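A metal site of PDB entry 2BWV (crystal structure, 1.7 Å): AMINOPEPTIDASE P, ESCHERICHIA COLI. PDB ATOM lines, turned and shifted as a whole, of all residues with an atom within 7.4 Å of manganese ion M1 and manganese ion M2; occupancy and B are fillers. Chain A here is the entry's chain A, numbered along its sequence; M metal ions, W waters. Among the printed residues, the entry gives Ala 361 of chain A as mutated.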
ATOM      1  N   TYR A 229       5.977  -8.950  22.835  1.00  0.00           N
ATOM      2  CA  TYR A 229       6.505  -7.687  23.352  1.00  0.00           C
ATOM      3  C   TYR A 229       6.122  -6.612  22.343  1.00  0.00           C
ATOM      4  O   TYR A 229       5.718  -6.916  21.237  1.00  0.00           O
ATOM      5  CB  TYR A 229       8.015  -7.718  23.531  1.00  0.00           C
ATOM      6  CG  TYR A 229       8.749  -8.137  22.290  1.00  0.00           C
ATOM      7  CD1 TYR A 229       8.971  -9.486  22.036  1.00  0.00           C
ATOM      8  CD2 TYR A 229       9.203  -7.203  21.337  1.00  0.00           C
ATOM      9  CE1 TYR A 229       9.616  -9.901  20.875  1.00  0.00           C
ATOM     10  CE2 TYR A 229       9.873  -7.616  20.173  1.00  0.00           C
ATOM     11  CZ  TYR A 229      10.083  -8.967  19.953  1.00  0.00           C
ATOM     12  OH  TYR A 229      10.728  -9.434  18.843  1.00  0.00           O
ATOM     13  N   ILE A 232       8.949  -3.116  17.594  1.00  0.00           N
ATOM     14  CA  ILE A 232       9.895  -2.031  17.307  1.00  0.00           C
ATOM     15  C   ILE A 232      10.080  -1.934  15.772  1.00  0.00           C
ATOM     16  O   ILE A 232      10.468  -2.905  15.125  1.00  0.00           O
ATOM     17  CB  ILE A 232      11.268  -2.366  17.954  1.00  0.00           C
ATOM     18  CG1 ILE A 232      11.143  -2.357  19.488  1.00  0.00           C
ATOM     19  CG2 ILE A 232      12.371  -1.436  17.453  1.00  0.00           C
ATOM     20  CD1 ILE A 232      12.170  -3.205  20.196  1.00  0.00           C
ATOM     21  N   ILE A 259      13.487  -3.871  12.410  1.00  0.00           N
ATOM     22  CA  ILE A 259      12.234  -4.396  12.932  1.00  0.00           C
ATOM     23  C   ILE A 259      12.556  -5.483  13.946  1.00  0.00           C
ATOM     24  O   ILE A 259      13.191  -6.505  13.604  1.00  0.00           O
ATOM     25  CB  ILE A 259      11.323  -4.952  11.834  1.00  0.00           C
ATOM     26  CG1 ILE A 259      10.984  -3.864  10.817  1.00  0.00           C
ATOM     27  CG2 ILE A 259      10.056  -5.499  12.440  1.00  0.00           C
ATOM     28  CD1 ILE A 259      10.004  -4.328   9.755  1.00  0.00           C
ATOM     29  N   ASP A 260      12.149  -5.245  15.186  1.00  0.00           N
ATOM     30  CA  ASP A 260      12.288  -6.235  16.254  1.00  0.00           C
ATOM     31  C   ASP A 260      10.858  -6.584  16.686  1.00  0.00           C
ATOM     32  O   ASP A 260      10.130  -5.737  17.199  1.00  0.00           O
ATOM     33  CB  ASP A 260      13.097  -5.662  17.408  1.00  0.00           C
ATOM     34  CG  ASP A 260      13.554  -6.744  18.386  1.00  0.00           C
ATOM     35  OD1 ASP A 260      13.000  -7.864  18.405  1.00  0.00           O
ATOM     36  OD2 ASP A 260      14.516  -6.468  19.143  1.00  0.00           O
ATOM     37  N   ALA A 261      10.433  -7.791  16.320  1.00  0.00           N
ATOM     38  CA  ALA A 261       9.037  -8.229  16.531  1.00  0.00           C
ATOM     39  C   ALA A 261       8.955  -9.726  16.722  1.00  0.00           C
ATOM     40  O   ALA A 261       9.696 -10.499  16.087  1.00  0.00           O
ATOM     41  CB  ALA A 261       8.147  -7.826  15.342  1.00  0.00           C
ATOM     42  N   GLY A 262       8.039 -10.127  17.586  1.00  0.00           N
ATOM     43  CA  GLY A 262       7.851 -11.527  17.936  1.00  0.00           C
ATOM     44  C   GLY A 262       6.429 -11.823  18.375  1.00  0.00           C
ATOM     45  O   GLY A 262       5.777 -11.008  19.022  1.00  0.00           O
ATOM     46  N   GLY A 270       8.243 -15.844  20.183  1.00  0.00           N
ATOM     47  CA  GLY A 270       9.246 -15.658  19.152  1.00  0.00           C
ATOM     48  C   GLY A 270       9.892 -14.291  19.376  1.00  0.00           C
ATOM     49  O   GLY A 270       9.352 -13.425  20.082  1.00  0.00           O
ATOM     50  N   ASP A 271      11.053 -14.088  18.763  1.00  0.00           N
ATOM     51  CA  ASP A 271      11.778 -12.855  18.939  1.00  0.00           C
ATOM     52  C   ASP A 271      12.805 -12.700  17.820  1.00  0.00           C
ATOM     53  O   ASP A 271      13.902 -13.221  17.900  1.00  0.00           O
ATOM     54  CB  ASP A 271      12.410 -12.837  20.326  1.00  0.00           C
ATOM     55  CG  ASP A 271      13.213 -11.578  20.620  1.00  0.00           C
ATOM     56  OD1 ASP A 271      13.226 -10.615  19.841  1.00  0.00           O
ATOM     57  OD2 ASP A 271      13.836 -11.545  21.697  1.00  0.00           O
ATOM     58  N   ILE A 272      12.432 -11.987  16.767  1.00  0.00           N
ATOM     59  CA  ILE A 272      13.307 -11.821  15.609  1.00  0.00           C
ATOM     60  C   ILE A 272      13.581 -10.331  15.392  1.00  0.00           C
ATOM     61  O   ILE A 272      12.677  -9.481  15.540  1.00  0.00           O
ATOM     62  CB  ILE A 272      12.676 -12.423  14.319  1.00  0.00           C
ATOM     63  CG1 ILE A 272      12.611 -13.961  14.377  1.00  0.00           C
ATOM     64  CG2 ILE A 272      13.403 -11.949  13.051  1.00  0.00           C
ATOM     65  CD1 ILE A 272      11.928 -14.574  13.151  1.00  0.00           C
ATOM     66  N   THR A 273      14.812 -10.023  15.016  1.00  0.00           N
ATOM     67  CA  THR A 273      15.148  -8.699  14.470  1.00  0.00           C
ATOM     68  C   THR A 273      15.745  -8.882  13.057  1.00  0.00           C
ATOM     69  O   THR A 273      16.609  -9.743  12.824  1.00  0.00           O
ATOM     70  CB  THR A 273      16.134  -7.870  15.335  1.00  0.00           C
ATOM     71  OG1 THR A 273      15.719  -7.842  16.709  1.00  0.00           O
ATOM     72  CG2 THR A 273      16.261  -6.412  14.803  1.00  0.00           C
ATOM     73  N   LEU A 352      24.519 -10.028  23.896  1.00  0.00           N
ATOM     74  CA  LEU A 352      24.375 -10.801  22.666  1.00  0.00           C
ATOM     75  C   LEU A 352      23.147 -11.734  22.696  1.00  0.00           C
ATOM     76  O   LEU A 352      22.572 -12.074  21.650  1.00  0.00           O
ATOM     77  CB  LEU A 352      25.617 -11.691  22.478  1.00  0.00           C
ATOM     78  CG  LEU A 352      25.673 -12.550  21.203  1.00  0.00           C
ATOM     79  CD1 LEU A 352      25.696 -11.686  19.942  1.00  0.00           C
ATOM     80  CD2 LEU A 352      26.896 -13.466  21.271  1.00  0.00           C
ATOM     81  N   SER A 353      22.784 -12.188  23.892  1.00  0.00           N
ATOM     82  CA  SER A 353      21.808 -13.261  24.037  1.00  0.00           C
ATOM     83  C   SER A 353      21.037 -13.174  25.325  1.00  0.00           C
ATOM     84  O   SER A 353      21.613 -12.880  26.379  1.00  0.00           O
ATOM     85  CB  SER A 353      22.520 -14.631  24.011  1.00  0.00           C
ATOM     86  OG  SER A 353      23.140 -14.861  22.761  1.00  0.00           O
ATOM     87  N   HIS A 354      19.751 -13.478  25.234  1.00  0.00           N
ATOM     88  CA  HIS A 354      18.947 -13.739  26.419  1.00  0.00           C
ATOM     89  C   HIS A 354      18.164 -15.029  26.244  1.00  0.00           C
ATOM     90  O   HIS A 354      17.847 -15.435  25.133  1.00  0.00           O
ATOM     91  CB  HIS A 354      17.995 -12.583  26.716  1.00  0.00           C
ATOM     92  CG  HIS A 354      17.045 -12.264  25.606  1.00  0.00           C
ATOM     93  ND1 HIS A 354      15.865 -12.951  25.407  1.00  0.00           N
ATOM     94  CD2 HIS A 354      17.116 -11.338  24.629  1.00  0.00           C
ATOM     95  CE1 HIS A 354      15.250 -12.453  24.344  1.00  0.00           C
ATOM     96  NE2 HIS A 354      15.993 -11.479  23.843  1.00  0.00           N
ATOM     97  N   TRP A 355      17.852 -15.660  27.367  1.00  0.00           N
ATOM     98  CA  TRP A 355      16.941 -16.806  27.367  1.00  0.00           C
ATOM     99  C   TRP A 355      15.589 -16.444  26.744  1.00  0.00           C
ATOM    100  O   TRP A 355      15.157 -15.279  26.799  1.00  0.00           O
ATOM    101  CB  TRP A 355      16.668 -17.308  28.786  1.00  0.00           C
ATOM    102  CG  TRP A 355      17.849 -17.550  29.686  1.00  0.00           C
ATOM    103  CD1 TRP A 355      17.999 -17.084  30.963  1.00  0.00           C
ATOM    104  CD2 TRP A 355      19.003 -18.373  29.419  1.00  0.00           C
ATOM    105  NE1 TRP A 355      19.176 -17.537  31.496  1.00  0.00           N
ATOM    106  CE2 TRP A 355      19.824 -18.328  30.583  1.00  0.00           C
ATOM    107  CE3 TRP A 355      19.436 -19.126  28.328  1.00  0.00           C
ATOM    108  CZ2 TRP A 355      21.038 -19.022  30.701  1.00  0.00           C
ATOM    109  CZ3 TRP A 355      20.669 -19.821  28.434  1.00  0.00           C
ATOM    110  CH2 TRP A 355      21.449 -19.753  29.613  1.00  0.00           C
ATOM    111  N   LEU A 356      14.912 -17.438  26.189  1.00  0.00           N
ATOM    112  CA  LEU A 356      13.640 -17.247  25.499  1.00  0.00           C
ATOM    113  C   LEU A 356      12.656 -18.346  25.944  1.00  0.00           C
ATOM    114  O   LEU A 356      13.033 -19.512  26.053  1.00  0.00           O
ATOM    115  CB  LEU A 356      13.851 -17.319  23.980  1.00  0.00           C
ATOM    116  CG  LEU A 356      12.669 -17.082  23.044  1.00  0.00           C
ATOM    117  CD1 LEU A 356      12.163 -15.641  23.136  1.00  0.00           C
ATOM    118  CD2 LEU A 356      13.055 -17.417  21.596  1.00  0.00           C
ATOM    119  N   VAL A 360       9.670 -13.301  26.801  1.00  0.00           N
ATOM    120  CA  VAL A 360      10.655 -13.031  25.779  1.00  0.00           C
ATOM    121  C   VAL A 360      12.048 -12.907  26.364  1.00  0.00           C
ATOM    122  O   VAL A 360      12.979 -13.508  25.833  1.00  0.00           O
ATOM    123  CB  VAL A 360      10.288 -11.821  24.847  1.00  0.00           C
ATOM    124  CG1 VAL A 360      10.155 -10.555  25.611  1.00  0.00           C
ATOM    125  CG2 VAL A 360      11.306 -11.719  23.721  1.00  0.00           C
ATOM    126  N   ALA A 361      12.192 -12.140  27.445  1.00  0.00           N
ATOM    127  CA  ALA A 361      13.446 -12.132  28.227  1.00  0.00           C
ATOM    128  C   ALA A 361      13.216 -13.146  29.360  1.00  0.00           C
ATOM    129  O   ALA A 361      12.738 -12.802  30.464  1.00  0.00           O
ATOM    130  CB  ALA A 361      13.758 -10.762  28.749  1.00  0.00           C
ATOM    131  N   LEU A 380      17.623 -19.596  23.527  1.00  0.00           N
ATOM    132  CA  LEU A 380      18.165 -18.242  23.657  1.00  0.00           C
ATOM    133  C   LEU A 380      18.173 -17.514  22.318  1.00  0.00           C
ATOM    134  O   LEU A 380      18.077 -18.125  21.234  1.00  0.00           O
ATOM    135  CB  LEU A 380      19.569 -18.237  24.269  1.00  0.00           C
ATOM    136  CG  LEU A 380      20.698 -19.005  23.516  1.00  0.00           C
ATOM    137  CD1 LEU A 380      22.105 -18.432  23.782  1.00  0.00           C
ATOM    138  CD2 LEU A 380      20.674 -20.513  23.816  1.00  0.00           C
ATOM    139  N   THR A 381      18.262 -16.188  22.414  1.00  0.00           N
ATOM    140  CA  THR A 381      18.392 -15.381  21.228  1.00  0.00           C
ATOM    141  C   THR A 381      19.863 -15.135  20.898  1.00  0.00           C
ATOM    142  O   THR A 381      20.734 -15.322  21.749  1.00  0.00           O
ATOM    143  CB  THR A 381      17.709 -14.010  21.402  1.00  0.00           C
ATOM    144  OG1 THR A 381      18.406 -13.275  22.419  1.00  0.00           O
ATOM    145  CG2 THR A 381      16.232 -14.160  21.778  1.00  0.00           C
ATOM    146  N   VAL A 382      20.124 -14.686  19.680  1.00  0.00           N
ATOM    147  CA  VAL A 382      21.458 -14.252  19.266  1.00  0.00           C
ATOM    148  C   VAL A 382      21.236 -12.971  18.491  1.00  0.00           C
ATOM    149  O   VAL A 382      20.648 -12.995  17.412  1.00  0.00           O
ATOM    150  CB  VAL A 382      22.174 -15.314  18.393  1.00  0.00           C
ATOM    151  CG1 VAL A 382      23.638 -14.923  18.137  1.00  0.00           C
ATOM    152  CG2 VAL A 382      22.066 -16.710  19.049  1.00  0.00           C
ATOM    153  N   GLU A 383      21.646 -11.842  19.057  1.00  0.00           N
ATOM    154  CA  GLU A 383      21.231 -10.525  18.552  1.00  0.00           C
ATOM    155  C   GLU A 383      22.329  -9.462  18.590  1.00  0.00           C
ATOM    156  O   GLU A 383      22.187  -8.415  19.238  1.00  0.00           O
ATOM    157  CB  GLU A 383      19.957 -10.058  19.263  1.00  0.00           C
ATOM    158  CG  GLU A 383      20.040  -9.897  20.745  1.00  0.00           C
ATOM    159  CD  GLU A 383      18.663  -9.593  21.295  1.00  0.00           C
ATOM    160  OE1 GLU A 383      18.059  -8.563  20.883  1.00  0.00           O
ATOM    161  OE2 GLU A 383      18.171 -10.405  22.095  1.00  0.00           O
ATOM    162  N   ARG A 404      20.505  -4.303  13.818  1.00  0.00           N
ATOM    163  CA  ARG A 404      20.518  -5.505  14.622  1.00  0.00           C
ATOM    164  C   ARG A 404      19.958  -6.661  13.804  1.00  0.00           C
ATOM    165  O   ARG A 404      19.032  -6.477  13.003  1.00  0.00           O
ATOM    166  CB  ARG A 404      19.729  -5.298  15.925  1.00  0.00           C
ATOM    167  CG  ARG A 404      19.549  -6.525  16.786  1.00  0.00           C
ATOM    168  CD  ARG A 404      19.103  -6.195  18.210  1.00  0.00           C
ATOM    169  NE  ARG A 404      17.723  -5.722  18.332  1.00  0.00           N
ATOM    170  CZ  ARG A 404      17.327  -4.452  18.503  1.00  0.00           C
ATOM    171  NH1 ARG A 404      18.204  -3.462  18.538  1.00  0.00           N
ATOM    172  NH2 ARG A 404      16.041  -4.133  18.630  1.00  0.00           N
ATOM    173  N   GLU A 406      18.733 -10.701  14.588  1.00  0.00           N
ATOM    174  CA  GLU A 406      18.460 -11.564  15.724  1.00  0.00           C
ATOM    175  C   GLU A 406      17.728 -12.830  15.312  1.00  0.00           C
ATOM    176  O   GLU A 406      16.685 -12.758  14.639  1.00  0.00           O
ATOM    177  CB  GLU A 406      17.649 -10.807  16.756  1.00  0.00           C
ATOM    178  CG  GLU A 406      17.070 -11.667  17.866  1.00  0.00           C
ATOM    179  CD  GLU A 406      16.339 -10.851  18.909  1.00  0.00           C
ATOM    180  OE1 GLU A 406      15.801  -9.759  18.591  1.00  0.00           O
ATOM    181  OE2 GLU A 406      16.317 -11.307  20.058  1.00  0.00           O
ATOM    182  N   ASP A 407      18.281 -13.983  15.727  1.00  0.00           N
ATOM    183  CA  ASP A 407      17.642 -15.304  15.553  1.00  0.00           C
ATOM    184  C   ASP A 407      17.407 -15.929  16.931  1.00  0.00           C
ATOM    185  O   ASP A 407      18.006 -15.510  17.936  1.00  0.00           O
ATOM    186  CB  ASP A 407      18.511 -16.239  14.700  1.00  0.00           C
ATOM    187  CG  ASP A 407      18.375 -15.990  13.189  1.00  0.00           C
ATOM    188  OD1 ASP A 407      17.302 -15.478  12.727  1.00  0.00           O
ATOM    189  OD2 ASP A 407      19.354 -16.316  12.478  1.00  0.00           O
ATOM    190  N   ASP A 408      16.495 -16.906  16.976  1.00  0.00           N
ATOM    191  CA  ASP A 408      16.195 -17.684  18.178  1.00  0.00           C
ATOM    192  C   ASP A 408      16.720 -19.096  17.944  1.00  0.00           C
ATOM    193  O   ASP A 408      16.475 -19.687  16.879  1.00  0.00           O
ATOM    194  CB  ASP A 408      14.697 -17.720  18.446  1.00  0.00           C
ATOM    195  CG  ASP A 408      14.084 -16.329  18.452  1.00  0.00           C
ATOM    196  OD1 ASP A 408      14.830 -15.396  18.840  1.00  0.00           O
ATOM    197  OD2 ASP A 408      12.901 -16.201  18.056  1.00  0.00           O
HETATM  198 MN    MN M   1      15.783 -10.639  21.894  1.00  0.00          MN
HETATM  199 MN    MN M   2      14.353  -8.903  19.886  1.00  0.00          MN
HETATM  200  O   HOH W   1      15.448  -8.687  21.511  1.00  0.00           O
HETATM  201  O   HOH W   2      12.759  -8.024  21.594  1.00  0.00           O
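O of Thr 273 is in hydrogen-bond range of N of Glu 406 (2.9 Å). OD1 of Asp 271 sits close to OH of Tyr 229 (2.9 Å). N of Asp 271 is in hydrogen-bond range of OD2 of Asp 408 (2.9 Å). O of His 354 is in hydrogen-bond range of N of Thr 381 (2.9 Å). O of Val 360 sits close to ND1 of His 354. The side-chain carboxylate of Asp 260 lies close to the side-chain hydroxyl of Thr 273. The side-chain carboxylate (OD1) of Asp 260 lies close to the side-chain hydroxyl (OH) of Tyr 229, at 2.8 Å. OH of Tyr 229 sits close to N of Ala 261 (3.0 Å).
Residues that only touch manganese ion M1: Thr 381 (3.6 Å). Five residues have an atom within 4 Å of manganese ion M1: Asp 271, His 354, Thr 381, Glu 383 and Glu 406. The nearest printed residue that does not touch manganese ion M1 is Val 360 (5.0 Å).
Merely in contact with manganese ion M2: Thr 273 (3.6 Å) and Tyr 229 (3.8 Å).
Manganese ion M1 is bound by water W1, OE2 of Glu 406, NE2 of His 354, OD2 of Asp 271 and OE2 of Glu 383.
Manganese ion M2 is bound by water W1, the side-chain carboxylate (OD1) of Asp 271, the side-chain carboxylate (OE1) of Glu 406, the side-chain carboxylate (OD1) of Asp 260, water W2 and the side-chain carboxylate (OD2) of Asp 260. Manganese ion M2 has six donor atoms within binding distance.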
